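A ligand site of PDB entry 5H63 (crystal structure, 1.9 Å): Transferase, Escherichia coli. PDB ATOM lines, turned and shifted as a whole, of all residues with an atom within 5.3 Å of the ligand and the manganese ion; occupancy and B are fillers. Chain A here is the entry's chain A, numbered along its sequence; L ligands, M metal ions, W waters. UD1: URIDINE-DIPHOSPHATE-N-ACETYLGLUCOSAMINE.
The side-chain carboxylate (OD1) of Asp 204 lies within hydrogen-bond range of an oxygen (O4') of the ligand (2.6 Å).
An oxygen (O1A) of the ligand lies within hydrogen-bond range of the backbone NH (N) of Ser 346.
The side-chain hydroxyl of Ser 346 lies within hydrogen-bond range of an oxygen (O1A) of the ligand.
O of Gln 64 sits at hydrogen-bond distance from O2' of the ligand, 2.6 Å away.
OH of Tyr 88 lies within hydrogen-bond range of O1A of the ligand (2.6 Å).
The side-chain carboxylate (OD2) of Asp 239 is in hydrogen-bond range of a nitrogen (N2') of the ligand (2.7 Å).
NH1 of Arg 207 sits at hydrogen-bond distance from O3' of the ligand, 2.7 Å away.
NE of Arg 348 is in salt-bridge range of O2B of the ligand, 2.8 Å away.
The backbone NH (N) of Phe 66 sits at hydrogen-bond distance from an oxygen (O2) of the ligand (3.0 Å).
A nitrogen (N3) of the ligand sits at hydrogen-bond distance from the backbone carbonyl oxygen (O) of Phe 66.
OG of Ser 345 lies within hydrogen-bond range of O2B of the ligand (2.9 Å).
The backbone NH (N) of Ala 240 lies within hydrogen-bond range of an oxygen (O3B) of the ligand (3.0 Å).
The backbone carbonyl oxygen (O) of Asn 272 sits close to a nitrogen (N2') of the ligand, 3.5 Å away.
The backbone NH of Gly 273 lies close to an oxygen (O3') of the ligand, 3.3 Å away.
The indole nitrogen of Trp 347 lies within hydrogen-bond range of an oxygen (O3A) of the ligand, 3.3 Å away.
ND1 of His 200 lies within hydrogen-bond range of O6' of the ligand (3.4 Å).
The side-chain hydroxyl of Tyr 237 sits at hydrogen-bond distance from an oxygen (O2') of the ligand.
The side-chain hydroxyl (OG1) of Thr 339 lies within hydrogen-bond range of the backbone carbonyl oxygen (O) of Asp 241, 2.8 Å away.
The side-chain carboxylate of Asp 204 sits at hydrogen-bond distance from a ring nitrogen (ND1) of His 200 (3.2 Å).
The side-chain amide oxygen of Gln 64 lies within hydrogen-bond range of the guanidinium group of Arg 207, at 2.8 Å.
NH1 of Arg 207 is in salt-bridge range of OD1 of Asp 239, at 3.6 Å.
The backbone carbonyl oxygen (O) of Gly 273 is in hydrogen-bond range of the backbone NH (N) of Asp 239, at 2.9 Å.
NH1 of Arg 207 sits at hydrogen-bond distance from OD1 of Asn 272, 2.9 Å away.
The guanidinium group of Arg 207 sits close to the side-chain hydroxyl of Tyr 237.
The indole nitrogen (NE1) of Trp 65 sits at hydrogen-bond distance from the side-chain carboxylate (OE2) of Glu 67 (2.9 Å).
Trp 65 touches the ligand (CH2 to C4, 3.3 Å).
Phe 203 touches the ligand (CE2 to O4B, 3.3 Å).
CE of Met 242 touches O7' of the ligand (3.96 Å).
CD2 of His 260 touches O7' of the ligand, 3.6 Å away.
Glu 271 touches the ligand.
Hydrophobic or aromatic side chains that line the ligand: Trp 65, Phe 66, Tyr 88, His 200, Phe 203, Ala 240, Met 242, His 260 and Trp 347.
23 residues have an atom within 4 Å of the ligand: Gln 64, Trp 65, Phe 66, Tyr 88, His 200, Phe 203, Asp 204, Arg 207, Tyr 237, Asp 239, Ala 240, Asp 241, Met 242, His 260, Glu 271, Asn 272, Gly 273, Asn 338, Ser 340, Ser 345, Ser 346, Trp 347 and Arg 348.
Of the 30 residues printed, 3 come within 4 Å of the manganese ion.
The manganese ion is bound by water W4 (2.1 Å), an oxygen (O1B) of the ligand (2.2 Å), the side-chain carboxylate of Asp 241 (2.2 Å), an oxygen (O2A) of the ligand (2.2 Å), the side-chain amide oxygen of Asn 338 (2.3 Å) and the side-chain hydroxyl of Ser 340 (2.5 Å).
Water W1 bridges O of Ser 346 (2.6 Å) and O4 of the ligand (2.7 Å).
Water W6 lies within hydrogen-bond range of O3B of the ligand (2.9 Å), N of Asp 241 (2.9 Å) and N of Ala 240 (3.2 Å).
Water W2 bridges O4 of the ligand and O of Phe 66.
Water W7 lies within hydrogen-bond range of O of Leu 238 (2.7 Å), N of Gln 64 (2.8 Å), O2' of the ligand (3.0 Å), OH of Tyr 237 (3.1 Å) and N of Ala 240 (3.3 Å).
Water W5 lies within hydrogen-bond range of ND2 of Asn 272 (2.7 Å), OD2 of Asp 204 (2.9 Å) and O6' of the ligand (3.5 Å).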
ATOM      1  N   GLN A  64     -27.941  34.596  -3.902  1.00  0.00           N
ATOM      2  CA  GLN A  64     -28.461  35.139  -5.124  1.00  0.00           C
ATOM      3  C   GLN A  64     -29.230  34.069  -5.898  1.00  0.00           C
ATOM      4  O   GLN A  64     -28.697  32.924  -6.060  1.00  0.00           O
ATOM      5  CB  GLN A  64     -27.308  35.661  -5.983  1.00  0.00           C
ATOM      6  CG  GLN A  64     -27.755  36.257  -7.342  1.00  0.00           C
ATOM      7  CD  GLN A  64     -26.580  36.777  -8.152  1.00  0.00           C
ATOM      8  OE1 GLN A  64     -25.508  36.217  -8.141  1.00  0.00           O
ATOM      9  NE2 GLN A  64     -26.812  37.895  -8.848  1.00  0.00           N
ATOM     10  N   TRP A  65     -30.404  34.418  -6.429  1.00  0.00           N
ATOM     11  CA  TRP A  65     -31.085  33.544  -7.398  1.00  0.00           C
ATOM     12  C   TRP A  65     -31.737  34.384  -8.512  1.00  0.00           C
ATOM     13  O   TRP A  65     -32.796  34.990  -8.296  1.00  0.00           O
ATOM     14  CB  TRP A  65     -32.094  32.528  -6.789  1.00  0.00           C
ATOM     15  CG  TRP A  65     -32.360  31.512  -7.778  1.00  0.00           C
ATOM     16  CD1 TRP A  65     -33.515  31.403  -8.496  1.00  0.00           C
ATOM     17  CD2 TRP A  65     -31.476  30.539  -8.300  1.00  0.00           C
ATOM     18  NE1 TRP A  65     -33.437  30.365  -9.385  1.00  0.00           N
ATOM     19  CE2 TRP A  65     -32.168  29.837  -9.309  1.00  0.00           C
ATOM     20  CE3 TRP A  65     -30.139  30.190  -8.028  1.00  0.00           C
ATOM     21  CZ2 TRP A  65     -31.582  28.794 -10.043  1.00  0.00           C
ATOM     22  CZ3 TRP A  65     -29.548  29.171  -8.730  1.00  0.00           C
ATOM     23  CH2 TRP A  65     -30.282  28.462  -9.754  1.00  0.00           C
ATOM     24  N   PHE A  66     -31.019  34.465  -9.641  1.00  0.00           N
ATOM     25  CA  PHE A  66     -31.519  35.085 -10.860  1.00  0.00           C
ATOM     26  C   PHE A  66     -32.113  33.987 -11.747  1.00  0.00           C
ATOM     27  O   PHE A  66     -31.445  33.033 -12.156  1.00  0.00           O
ATOM     28  CB  PHE A  66     -30.392  35.846 -11.556  1.00  0.00           C
ATOM     29  CG  PHE A  66     -30.109  37.207 -10.991  1.00  0.00           C
ATOM     30  CD1 PHE A  66     -30.439  37.540  -9.668  1.00  0.00           C
ATOM     31  CD2 PHE A  66     -29.592  38.215 -11.822  1.00  0.00           C
ATOM     32  CE1 PHE A  66     -30.187  38.816  -9.136  1.00  0.00           C
ATOM     33  CE2 PHE A  66     -29.369  39.510 -11.301  1.00  0.00           C
ATOM     34  CZ  PHE A  66     -29.673  39.801  -9.962  1.00  0.00           C
ATOM     35  N   GLU A  67     -33.387  34.124 -12.057  1.00  0.00           N
ATOM     36  CA  GLU A  67     -34.105  33.009 -12.652  1.00  0.00           C
ATOM     37  C   GLU A  67     -34.558  33.394 -14.041  1.00  0.00           C
ATOM     38  O   GLU A  67     -35.449  34.229 -14.180  1.00  0.00           O
ATOM     39  CB  GLU A  67     -35.289  32.636 -11.750  1.00  0.00           C
ATOM     40  CG  GLU A  67     -36.157  31.526 -12.356  1.00  0.00           C
ATOM     41  CD  GLU A  67     -35.371  30.299 -12.777  1.00  0.00           C
ATOM     42  OE1 GLU A  67     -35.414  29.938 -13.970  1.00  0.00           O
ATOM     43  OE2 GLU A  67     -34.705  29.654 -11.936  1.00  0.00           O
ATOM     44  N   ARG A  72     -40.936  27.689 -15.247  1.00  0.00           N
ATOM     45  CA  ARG A  72     -40.655  26.315 -14.880  1.00  0.00           C
ATOM     46  C   ARG A  72     -41.048  25.919 -13.430  1.00  0.00           C
ATOM     47  O   ARG A  72     -41.067  24.741 -13.059  1.00  0.00           O
ATOM     48  CB  ARG A  72     -39.196  25.973 -15.230  1.00  0.00           C
ATOM     49  CG  ARG A  72     -38.141  26.338 -14.189  1.00  0.00           C
ATOM     50  CD  ARG A  72     -36.752  26.331 -14.819  1.00  0.00           C
ATOM     51  NE  ARG A  72     -35.772  26.937 -13.900  1.00  0.00           N
ATOM     52  CZ  ARG A  72     -34.697  26.352 -13.393  1.00  0.00           C
ATOM     53  NH1 ARG A  72     -34.364  25.105 -13.730  1.00  0.00           N
ATOM     54  NH2 ARG A  72     -33.919  27.059 -12.549  1.00  0.00           N
ATOM     55  N   ASN A  86     -29.502  20.126  -7.082  1.00  0.00           N
ATOM     56  CA  ASN A  86     -29.288  21.562  -6.740  1.00  0.00           C
ATOM     57  C   ASN A  86     -30.319  21.996  -5.670  1.00  0.00           C
ATOM     58  O   ASN A  86     -31.299  22.653  -6.005  1.00  0.00           O
ATOM     59  CB  ASN A  86     -29.417  22.427  -7.988  1.00  0.00           C
ATOM     60  CG  ASN A  86     -28.314  22.159  -9.015  1.00  0.00           C
ATOM     61  OD1 ASN A  86     -28.631  21.754 -10.116  1.00  0.00           O
ATOM     62  ND2 ASN A  86     -27.068  22.364  -8.656  1.00  0.00           N
ATOM     63  N   TYR A  88     -30.980  24.245  -3.658  1.00  0.00           N
ATOM     64  CA  TYR A  88     -30.513  25.587  -3.227  1.00  0.00           C
ATOM     65  C   TYR A  88     -31.396  26.353  -2.248  1.00  0.00           C
ATOM     66  O   TYR A  88     -30.899  26.959  -1.307  1.00  0.00           O
ATOM     67  CB  TYR A  88     -30.062  26.395  -4.427  1.00  0.00           C
ATOM     68  CG  TYR A  88     -28.830  25.873  -5.192  1.00  0.00           C
ATOM     69  CD1 TYR A  88     -28.092  24.771  -4.759  1.00  0.00           C
ATOM     70  CD2 TYR A  88     -28.425  26.468  -6.379  1.00  0.00           C
ATOM     71  CE1 TYR A  88     -26.960  24.313  -5.434  1.00  0.00           C
ATOM     72  CE2 TYR A  88     -27.268  26.048  -7.035  1.00  0.00           C
ATOM     73  CZ  TYR A  88     -26.574  24.906  -6.578  1.00  0.00           C
ATOM     74  OH  TYR A  88     -25.463  24.448  -7.289  1.00  0.00           O
ATOM     75  N   HIS A 200     -24.651  33.271 -17.553  1.00  0.00           N
ATOM     76  CA  HIS A 200     -24.065  33.512 -16.236  1.00  0.00           C
ATOM     77  C   HIS A 200     -23.612  34.960 -16.032  1.00  0.00           C
ATOM     78  O   HIS A 200     -23.510  35.417 -14.906  1.00  0.00           O
ATOM     79  CB  HIS A 200     -22.887  32.573 -15.915  1.00  0.00           C
ATOM     80  CG  HIS A 200     -21.674  32.830 -16.734  1.00  0.00           C
ATOM     81  ND1 HIS A 200     -20.656  33.637 -16.309  1.00  0.00           N
ATOM     82  CD2 HIS A 200     -21.365  32.478 -18.003  1.00  0.00           C
ATOM     83  CE1 HIS A 200     -19.750  33.728 -17.268  1.00  0.00           C
ATOM     84  NE2 HIS A 200     -20.150  33.030 -18.302  1.00  0.00           N
ATOM     85  N   PHE A 203     -26.201  37.184 -13.714  1.00  0.00           N
ATOM     86  CA  PHE A 203     -26.017  37.137 -12.245  1.00  0.00           C
ATOM     87  C   PHE A 203     -24.622  37.556 -11.802  1.00  0.00           C
ATOM     88  O   PHE A 203     -24.503  38.272 -10.796  1.00  0.00           O
ATOM     89  CB  PHE A 203     -26.492  35.852 -11.576  1.00  0.00           C
ATOM     90  CG  PHE A 203     -26.144  34.582 -12.274  1.00  0.00           C
ATOM     91  CD1 PHE A 203     -27.038  34.002 -13.148  1.00  0.00           C
ATOM     92  CD2 PHE A 203     -25.014  33.914 -11.950  1.00  0.00           C
ATOM     93  CE1 PHE A 203     -26.763  32.761 -13.734  1.00  0.00           C
ATOM     94  CE2 PHE A 203     -24.716  32.677 -12.479  1.00  0.00           C
ATOM     95  CZ  PHE A 203     -25.573  32.090 -13.390  1.00  0.00           C
ATOM     96  N   ASP A 204     -23.581  37.196 -12.526  1.00  0.00           N
ATOM     97  CA  ASP A 204     -22.210  37.586 -12.108  1.00  0.00           C
ATOM     98  C   ASP A 204     -21.997  39.099 -12.063  1.00  0.00           C
ATOM     99  O   ASP A 204     -21.398  39.627 -11.113  1.00  0.00           O
ATOM    100  CB  ASP A 204     -21.129  36.912 -12.941  1.00  0.00           C
ATOM    101  CG  ASP A 204     -21.013  35.447 -12.649  1.00  0.00           C
ATOM    102  OD1 ASP A 204     -21.718  34.946 -11.723  1.00  0.00           O
ATOM    103  OD2 ASP A 204     -20.258  34.807 -13.380  1.00  0.00           O
ATOM    104  N   ARG A 207     -24.223  40.670  -9.200  1.00  0.00           N
ATOM    105  CA  ARG A 207     -23.645  40.328  -7.872  1.00  0.00           C
ATOM    106  C   ARG A 207     -22.607  41.382  -7.433  1.00  0.00           C
ATOM    107  O   ARG A 207     -22.653  41.865  -6.308  1.00  0.00           O
ATOM    108  CB  ARG A 207     -23.083  38.899  -7.924  1.00  0.00           C
ATOM    109  CG  ARG A 207     -22.451  38.431  -6.622  1.00  0.00           C
ATOM    110  CD  ARG A 207     -21.834  37.081  -6.829  1.00  0.00           C
ATOM    111  NE  ARG A 207     -22.765  36.132  -7.447  1.00  0.00           N
ATOM    112  CZ  ARG A 207     -22.398  34.975  -7.994  1.00  0.00           C
ATOM    113  NH1 ARG A 207     -21.133  34.633  -8.120  1.00  0.00           N
ATOM    114  NH2 ARG A 207     -23.347  34.191  -8.546  1.00  0.00           N
ATOM    115  N   TYR A 237     -21.352  37.530   0.661  1.00  0.00           N
ATOM    116  CA  TYR A 237     -21.977  36.827  -0.456  1.00  0.00           C
ATOM    117  C   TYR A 237     -21.507  35.381  -0.510  1.00  0.00           C
ATOM    118  O   TYR A 237     -20.258  35.132  -0.515  1.00  0.00           O
ATOM    119  CB  TYR A 237     -21.629  37.496  -1.804  1.00  0.00           C
ATOM    120  CG  TYR A 237     -22.123  36.611  -2.863  1.00  0.00           C
ATOM    121  CD1 TYR A 237     -23.458  36.578  -3.189  1.00  0.00           C
ATOM    122  CD2 TYR A 237     -21.269  35.645  -3.412  1.00  0.00           C
ATOM    123  CE1 TYR A 237     -23.924  35.624  -4.086  1.00  0.00           C
ATOM    124  CE2 TYR A 237     -21.726  34.686  -4.282  1.00  0.00           C
ATOM    125  CZ  TYR A 237     -23.057  34.693  -4.638  1.00  0.00           C
ATOM    126  OH  TYR A 237     -23.526  33.707  -5.512  1.00  0.00           O
ATOM    127  N   LEU A 238     -22.457  34.477  -0.658  1.00  0.00           N
ATOM    128  CA  LEU A 238     -22.195  33.016  -0.839  1.00  0.00           C
ATOM    129  C   LEU A 238     -23.034  32.462  -1.953  1.00  0.00           C
ATOM    130  O   LEU A 238     -24.276  32.708  -1.984  1.00  0.00           O
ATOM    131  CB  LEU A 238     -22.531  32.221   0.426  1.00  0.00           C
ATOM    132  CG  LEU A 238     -21.861  32.578   1.708  1.00  0.00           C
ATOM    133  CD1 LEU A 238     -22.544  31.792   2.809  1.00  0.00           C
ATOM    134  CD2 LEU A 238     -20.385  32.347   1.788  1.00  0.00           C
ATOM    135  N   ASP A 239     -22.410  31.692  -2.821  1.00  0.00           N
ATOM    136  CA  ASP A 239     -23.115  30.759  -3.705  1.00  0.00           C
ATOM    137  C   ASP A 239     -24.004  29.826  -2.822  1.00  0.00           C
ATOM    138  O   ASP A 239     -23.605  29.412  -1.744  1.00  0.00           O
ATOM    139  CB  ASP A 239     -22.127  29.889  -4.493  1.00  0.00           C
ATOM    140  CG  ASP A 239     -21.509  30.594  -5.725  1.00  0.00           C
ATOM    141  OD1 ASP A 239     -21.862  31.768  -6.047  1.00  0.00           O
ATOM    142  OD2 ASP A 239     -20.693  29.942  -6.430  1.00  0.00           O
ATOM    143  N   ALA A 240     -25.163  29.457  -3.319  1.00  0.00           N
ATOM    144  CA  ALA A 240     -26.139  28.684  -2.569  1.00  0.00           C
ATOM    145  C   ALA A 240     -25.716  27.253  -2.277  1.00  0.00           C
ATOM    146  O   ALA A 240     -26.341  26.615  -1.471  1.00  0.00           O
ATOM    147  CB  ALA A 240     -27.488  28.721  -3.285  1.00  0.00           C
ATOM    148  N   ASP A 241     -24.626  26.762  -2.885  1.00  0.00           N
ATOM    149  CA  ASP A 241     -24.055  25.463  -2.534  1.00  0.00           C
ATOM    150  C   ASP A 241     -22.865  25.535  -1.529  1.00  0.00           C
ATOM    151  O   ASP A 241     -22.173  24.532  -1.353  1.00  0.00           O
ATOM    152  CB  ASP A 241     -23.603  24.802  -3.827  1.00  0.00           C
ATOM    153  CG  ASP A 241     -22.342  25.485  -4.444  1.00  0.00           C
ATOM    154  OD1 ASP A 241     -21.989  26.649  -4.079  1.00  0.00           O
ATOM    155  OD2 ASP A 241     -21.782  24.865  -5.354  1.00  0.00           O
ATOM    156  N   MET A 242     -22.584  26.711  -0.976  1.00  0.00           N
ATOM    157  CA  MET A 242     -21.610  26.898   0.070  1.00  0.00           C
ATOM    158  C   MET A 242     -22.363  26.564   1.392  1.00  0.00           C
ATOM    159  O   MET A 242     -23.091  27.389   1.956  1.00  0.00           O
ATOM    160  CB  MET A 242     -21.091  28.372   0.069  1.00  0.00           C
ATOM    161  CG  MET A 242     -20.422  28.833  -1.212  1.00  0.00           C
ATOM    162  SD  MET A 242     -18.775  28.157  -1.348  1.00  0.00           S
ATOM    163  CE  MET A 242     -18.194  28.740  -2.961  1.00  0.00           C
ATOM    164  N   HIS A 260     -13.396  33.697  -2.356  1.00  0.00           N
ATOM    165  CA  HIS A 260     -13.158  32.278  -2.502  1.00  0.00           C
ATOM    166  C   HIS A 260     -11.849  31.986  -3.286  1.00  0.00           C
ATOM    167  O   HIS A 260     -11.538  32.671  -4.301  1.00  0.00           O
ATOM    168  CB  HIS A 260     -14.368  31.628  -3.210  1.00  0.00           C
ATOM    169  CG  HIS A 260     -14.299  30.152  -3.368  1.00  0.00           C
ATOM    170  ND1 HIS A 260     -13.916  29.290  -2.367  1.00  0.00           N
ATOM    171  CD2 HIS A 260     -14.689  29.374  -4.407  1.00  0.00           C
ATOM    172  CE1 HIS A 260     -14.030  28.040  -2.798  1.00  0.00           C
ATOM    173  NE2 HIS A 260     -14.501  28.070  -4.043  1.00  0.00           N
ATOM    174  N   GLU A 271     -11.619  32.633  -7.226  1.00  0.00           N
ATOM    175  CA  GLU A 271     -12.901  32.175  -7.755  1.00  0.00           C
ATOM    176  C   GLU A 271     -13.943  33.104  -7.294  1.00  0.00           C
ATOM    177  O   GLU A 271     -13.810  33.771  -6.302  1.00  0.00           O
ATOM    178  CB  GLU A 271     -13.231  30.794  -7.244  1.00  0.00           C
ATOM    179  CG  GLU A 271     -12.223  29.738  -7.645  1.00  0.00           C
ATOM    180  CD  GLU A 271     -12.164  29.453  -9.121  1.00  0.00           C
ATOM    181  OE1 GLU A 271     -11.282  28.671  -9.460  1.00  0.00           O
ATOM    182  OE2 GLU A 271     -12.925  29.971  -9.943  1.00  0.00           O
ATOM    183  N   ASN A 272     -15.003  33.135  -8.065  1.00  0.00           N
ATOM    184  CA  ASN A 272     -16.188  33.720  -7.642  1.00  0.00           C
ATOM    185  C   ASN A 272     -16.794  32.753  -6.604  1.00  0.00           C
ATOM    186  O   ASN A 272     -16.401  31.566  -6.542  1.00  0.00           O
ATOM    187  CB  ASN A 272     -17.084  33.902  -8.874  1.00  0.00           C
ATOM    188  CG  ASN A 272     -17.985  35.077  -8.701  1.00  0.00           C
ATOM    189  OD1 ASN A 272     -18.384  35.382  -7.538  1.00  0.00           O
ATOM    190  ND2 ASN A 272     -18.382  35.680  -9.795  1.00  0.00           N
ATOM    191  N   GLY A 273     -17.776  33.193  -5.884  1.00  0.00           N
ATOM    192  CA  GLY A 273     -18.621  32.247  -5.146  1.00  0.00           C
ATOM    193  C   GLY A 273     -18.652  32.498  -3.661  1.00  0.00           C
ATOM    194  O   GLY A 273     -19.572  32.038  -2.989  1.00  0.00           O
ATOM    195  N   ASN A 338     -18.590  25.050  -2.445  1.00  0.00           N
ATOM    196  CA  ASN A 338     -18.761  24.686  -3.872  1.00  0.00           C
ATOM    197  C   ASN A 338     -19.213  23.221  -3.999  1.00  0.00           C
ATOM    198  O   ASN A 338     -18.608  22.421  -4.742  1.00  0.00           O
ATOM    199  CB  ASN A 338     -17.468  24.942  -4.699  1.00  0.00           C
ATOM    200  CG  ASN A 338     -17.702  24.825  -6.190  1.00  0.00           C
ATOM    201  OD1 ASN A 338     -18.834  24.676  -6.643  1.00  0.00           O
ATOM    202  ND2 ASN A 338     -16.634  24.872  -6.972  1.00  0.00           N
ATOM    203  N   THR A 339     -20.279  22.881  -3.287  1.00  0.00           N
ATOM    204  CA  THR A 339     -20.750  21.485  -3.325  1.00  0.00           C
ATOM    205  C   THR A 339     -21.349  21.052  -4.648  1.00  0.00           C
ATOM    206  O   THR A 339     -21.462  19.852  -4.914  1.00  0.00           O
ATOM    207  CB  THR A 339     -21.710  21.151  -2.178  1.00  0.00           C
ATOM    208  OG1 THR A 339     -22.896  21.949  -2.254  1.00  0.00           O
ATOM    209  CG2 THR A 339     -21.041  21.323  -0.858  1.00  0.00           C
ATOM    210  N   SER A 340     -21.689  21.983  -5.504  1.00  0.00           N
ATOM    211  CA  SER A 340     -22.148  21.634  -6.831  1.00  0.00           C
ATOM    212  C   SER A 340     -21.066  20.880  -7.654  1.00  0.00           C
ATOM    213  O   SER A 340     -21.389  20.096  -8.459  1.00  0.00           O
ATOM    214  CB  SER A 340     -22.610  22.862  -7.594  1.00  0.00           C
ATOM    215  OG  SER A 340     -21.575  23.504  -8.177  1.00  0.00           O
ATOM    216  N   SER A 341     -19.796  21.160  -7.443  1.00  0.00           N
ATOM    217  CA  SER A 341     -18.740  20.515  -8.207  1.00  0.00           C
ATOM    218  C   SER A 341     -18.602  19.054  -7.858  1.00  0.00           C
ATOM    219  O   SER A 341     -17.881  18.346  -8.483  1.00  0.00           O
ATOM    220  CB  SER A 341     -17.430  21.249  -8.140  1.00  0.00           C
ATOM    221  OG  SER A 341     -16.993  21.348  -6.862  1.00  0.00           O
ATOM    222  N   ALA A 344     -23.859  18.679  -9.454  1.00  0.00           N
ATOM    223  CA  ALA A 344     -23.966  19.328 -10.768  1.00  0.00           C
ATOM    224  C   ALA A 344     -24.199  20.824 -10.768  1.00  0.00           C
ATOM    225  O   ALA A 344     -25.022  21.333 -10.069  1.00  0.00           O
ATOM    226  CB  ALA A 344     -25.020  18.674 -11.643  1.00  0.00           C
ATOM    227  N   SER A 345     -23.537  21.475 -11.701  1.00  0.00           N
ATOM    228  CA  SER A 345     -23.682  22.935 -11.937  1.00  0.00           C
ATOM    229  C   SER A 345     -25.134  23.283 -12.307  1.00  0.00           C
ATOM    230  O   SER A 345     -25.753  22.647 -13.186  1.00  0.00           O
ATOM    231  CB  SER A 345     -22.751  23.368 -13.091  1.00  0.00           C
ATOM    232  OG  SER A 345     -21.950  24.486 -12.746  1.00  0.00           O
ATOM    233  N   SER A 346     -25.673  24.316 -11.646  1.00  0.00           N
ATOM    234  CA  SER A 346     -27.060  24.745 -11.885  1.00  0.00           C
ATOM    235  C   SER A 346     -27.270  25.468 -13.230  1.00  0.00           C
ATOM    236  O   SER A 346     -28.413  25.769 -13.540  1.00  0.00           O
ATOM    237  CB  SER A 346     -27.463  25.707 -10.786  1.00  0.00           C
ATOM    238  OG  SER A 346     -26.504  26.713 -10.753  1.00  0.00           O
ATOM    239  N   TRP A 347     -26.186  25.801 -13.964  1.00  0.00           N
ATOM    240  CA  TRP A 347     -26.245  26.583 -15.246  1.00  0.00           C
ATOM    241  C   TRP A 347     -25.243  26.177 -16.383  1.00  0.00           C
ATOM    242  O   TRP A 347     -25.311  26.746 -17.467  1.00  0.00           O
ATOM    243  CB  TRP A 347     -26.024  28.089 -14.945  1.00  0.00           C
ATOM    244  CG  TRP A 347     -24.623  28.297 -14.482  1.00  0.00           C
ATOM    245  CD1 TRP A 347     -24.140  28.112 -13.223  1.00  0.00           C
ATOM    246  CD2 TRP A 347     -23.501  28.560 -15.320  1.00  0.00           C
ATOM    247  NE1 TRP A 347     -22.799  28.288 -13.205  1.00  0.00           N
ATOM    248  CE2 TRP A 347     -22.364  28.561 -14.481  1.00  0.00           C
ATOM    249  CE3 TRP A 347     -23.335  28.811 -16.708  1.00  0.00           C
ATOM    250  CZ2 TRP A 347     -21.078  28.836 -14.970  1.00  0.00           C
ATOM    251  CZ3 TRP A 347     -22.050  29.070 -17.185  1.00  0.00           C
ATOM    252  CH2 TRP A 347     -20.930  29.089 -16.308  1.00  0.00           C
ATOM    253  N   ARG A 348     -24.319  25.246 -16.151  1.00  0.00           N
ATOM    254  CA  ARG A 348     -23.294  24.924 -17.191  1.00  0.00           C
ATOM    255  C   ARG A 348     -23.811  23.935 -18.257  1.00  0.00           C
ATOM    256  O   ARG A 348     -24.342  22.864 -17.942  1.00  0.00           O
ATOM    257  CB  ARG A 348     -21.971  24.434 -16.560  1.00  0.00           C
ATOM    258  CG  ARG A 348     -21.200  25.540 -15.838  1.00  0.00           C
ATOM    259  CD  ARG A 348     -19.942  25.000 -15.149  1.00  0.00           C
ATOM    260  NE  ARG A 348     -19.393  25.947 -14.168  1.00  0.00           N
ATOM    261  CZ  ARG A 348     -18.629  27.012 -14.445  1.00  0.00           C
ATOM    262  NH1 ARG A 348     -18.331  27.330 -15.712  1.00  0.00           N
ATOM    263  NH2 ARG A 348     -18.210  27.801 -13.455  1.00  0.00           N
HETATM  264  C1' UD1 L   1     -19.608  29.192 -10.509  1.00  0.00           C
HETATM  265  C2' UD1 L   1     -19.157  30.216  -9.422  1.00  0.00           C
HETATM  266  C3' UD1 L   1     -20.289  31.207  -9.172  1.00  0.00           C
HETATM  267  C4' UD1 L   1     -20.524  31.889 -10.508  1.00  0.00           C
HETATM  268  C5' UD1 L   1     -20.857  30.835 -11.586  1.00  0.00           C
HETATM  269  C6' UD1 L   1     -21.126  31.489 -12.947  1.00  0.00           C
HETATM  270  C7' UD1 L   1     -17.531  29.001  -7.934  1.00  0.00           C
HETATM  271  C8' UD1 L   1     -16.584  28.964  -9.040  1.00  0.00           C
HETATM  272  N2' UD1 L   1     -18.690  29.568  -8.178  1.00  0.00           N
HETATM  273  O1' UD1 L   1     -20.801  28.467 -10.120  1.00  0.00           O
HETATM  274  O3' UD1 L   1     -19.970  32.155  -8.151  1.00  0.00           O
HETATM  275  O4' UD1 L   1     -21.688  32.681 -10.506  1.00  0.00           O
HETATM  276  O5' UD1 L   1     -19.782  29.922 -11.725  1.00  0.00           O
HETATM  277  O6' UD1 L   1     -19.939  32.090 -13.367  1.00  0.00           O
HETATM  278  O7' UD1 L   1     -17.244  28.469  -6.792  1.00  0.00           O
HETATM  279  N1  UD1 L   1     -27.094  31.163 -10.311  1.00  0.00           N
HETATM  280  C2  UD1 L   1     -28.243  31.917 -10.622  1.00  0.00           C
HETATM  281  N3  UD1 L   1     -29.129  31.497 -11.517  1.00  0.00           N
HETATM  282  C4  UD1 L   1     -28.928  30.332 -12.162  1.00  0.00           C
HETATM  283  C5  UD1 L   1     -27.803  29.558 -11.896  1.00  0.00           C
HETATM  284  C6  UD1 L   1     -26.873  29.987 -10.951  1.00  0.00           C
HETATM  285  O2  UD1 L   1     -28.465  33.003 -10.002  1.00  0.00           O
HETATM  286  O4  UD1 L   1     -29.754  29.987 -13.033  1.00  0.00           O
HETATM  287  C1B UD1 L   1     -26.168  31.722  -9.312  1.00  0.00           C
HETATM  288  C2B UD1 L   1     -26.603  31.401  -7.900  1.00  0.00           C
HETATM  289  O2' UD1 L   1     -26.311  32.518  -7.091  1.00  0.00           O
HETATM  290  C3B UD1 L   1     -25.771  30.177  -7.550  1.00  0.00           C
HETATM  291  C4B UD1 L   1     -24.508  30.499  -8.311  1.00  0.00           C
HETATM  292  O4B UD1 L   1     -24.910  31.177  -9.523  1.00  0.00           O
HETATM  293  O3B UD1 L   1     -25.442  30.112  -6.186  1.00  0.00           O
HETATM  294  C5B UD1 L   1     -23.620  29.323  -8.569  1.00  0.00           C
HETATM  295  O5B UD1 L   1     -24.317  28.185  -9.075  1.00  0.00           O
HETATM  296  PA  UD1 L   1     -23.458  26.836  -8.985  1.00  0.00           P
HETATM  297  O1A UD1 L   1     -24.506  25.840  -9.316  1.00  0.00           O
HETATM  298  O2A UD1 L   1     -22.712  26.745  -7.703  1.00  0.00           O
HETATM  299  O3A UD1 L   1     -22.440  26.846 -10.236  1.00  0.00           O
HETATM  300  PB  UD1 L   1     -20.850  26.837 -10.249  1.00  0.00           P
HETATM  301  O1B UD1 L   1     -20.115  26.342  -9.102  1.00  0.00           O
HETATM  302  O2B UD1 L   1     -20.348  26.600 -11.590  1.00  0.00           O
HETATM  303 MN    MN M   1     -20.852  25.642  -7.181  1.00  0.00          MN
HETATM  304  O   HOH W   1     -30.370  27.433 -13.568  1.00  0.00           O
HETATM  305  O   HOH W   2     -31.626  31.189 -14.883  1.00  0.00           O
HETATM  306  O   HOH W   3     -17.588  25.057  -9.680  1.00  0.00           O
HETATM  307  O   HOH W   4     -20.295  27.264  -5.991  1.00  0.00           O
HETATM  308  O   HOH W   5     -17.702  34.413 -12.055  1.00  0.00           O
HETATM  309  O   HOH W   6     -24.504  27.458  -5.682  1.00  0.00           O
HETATM  310  O   HOH W   7     -26.008  32.528  -4.059  1.00  0.00           O
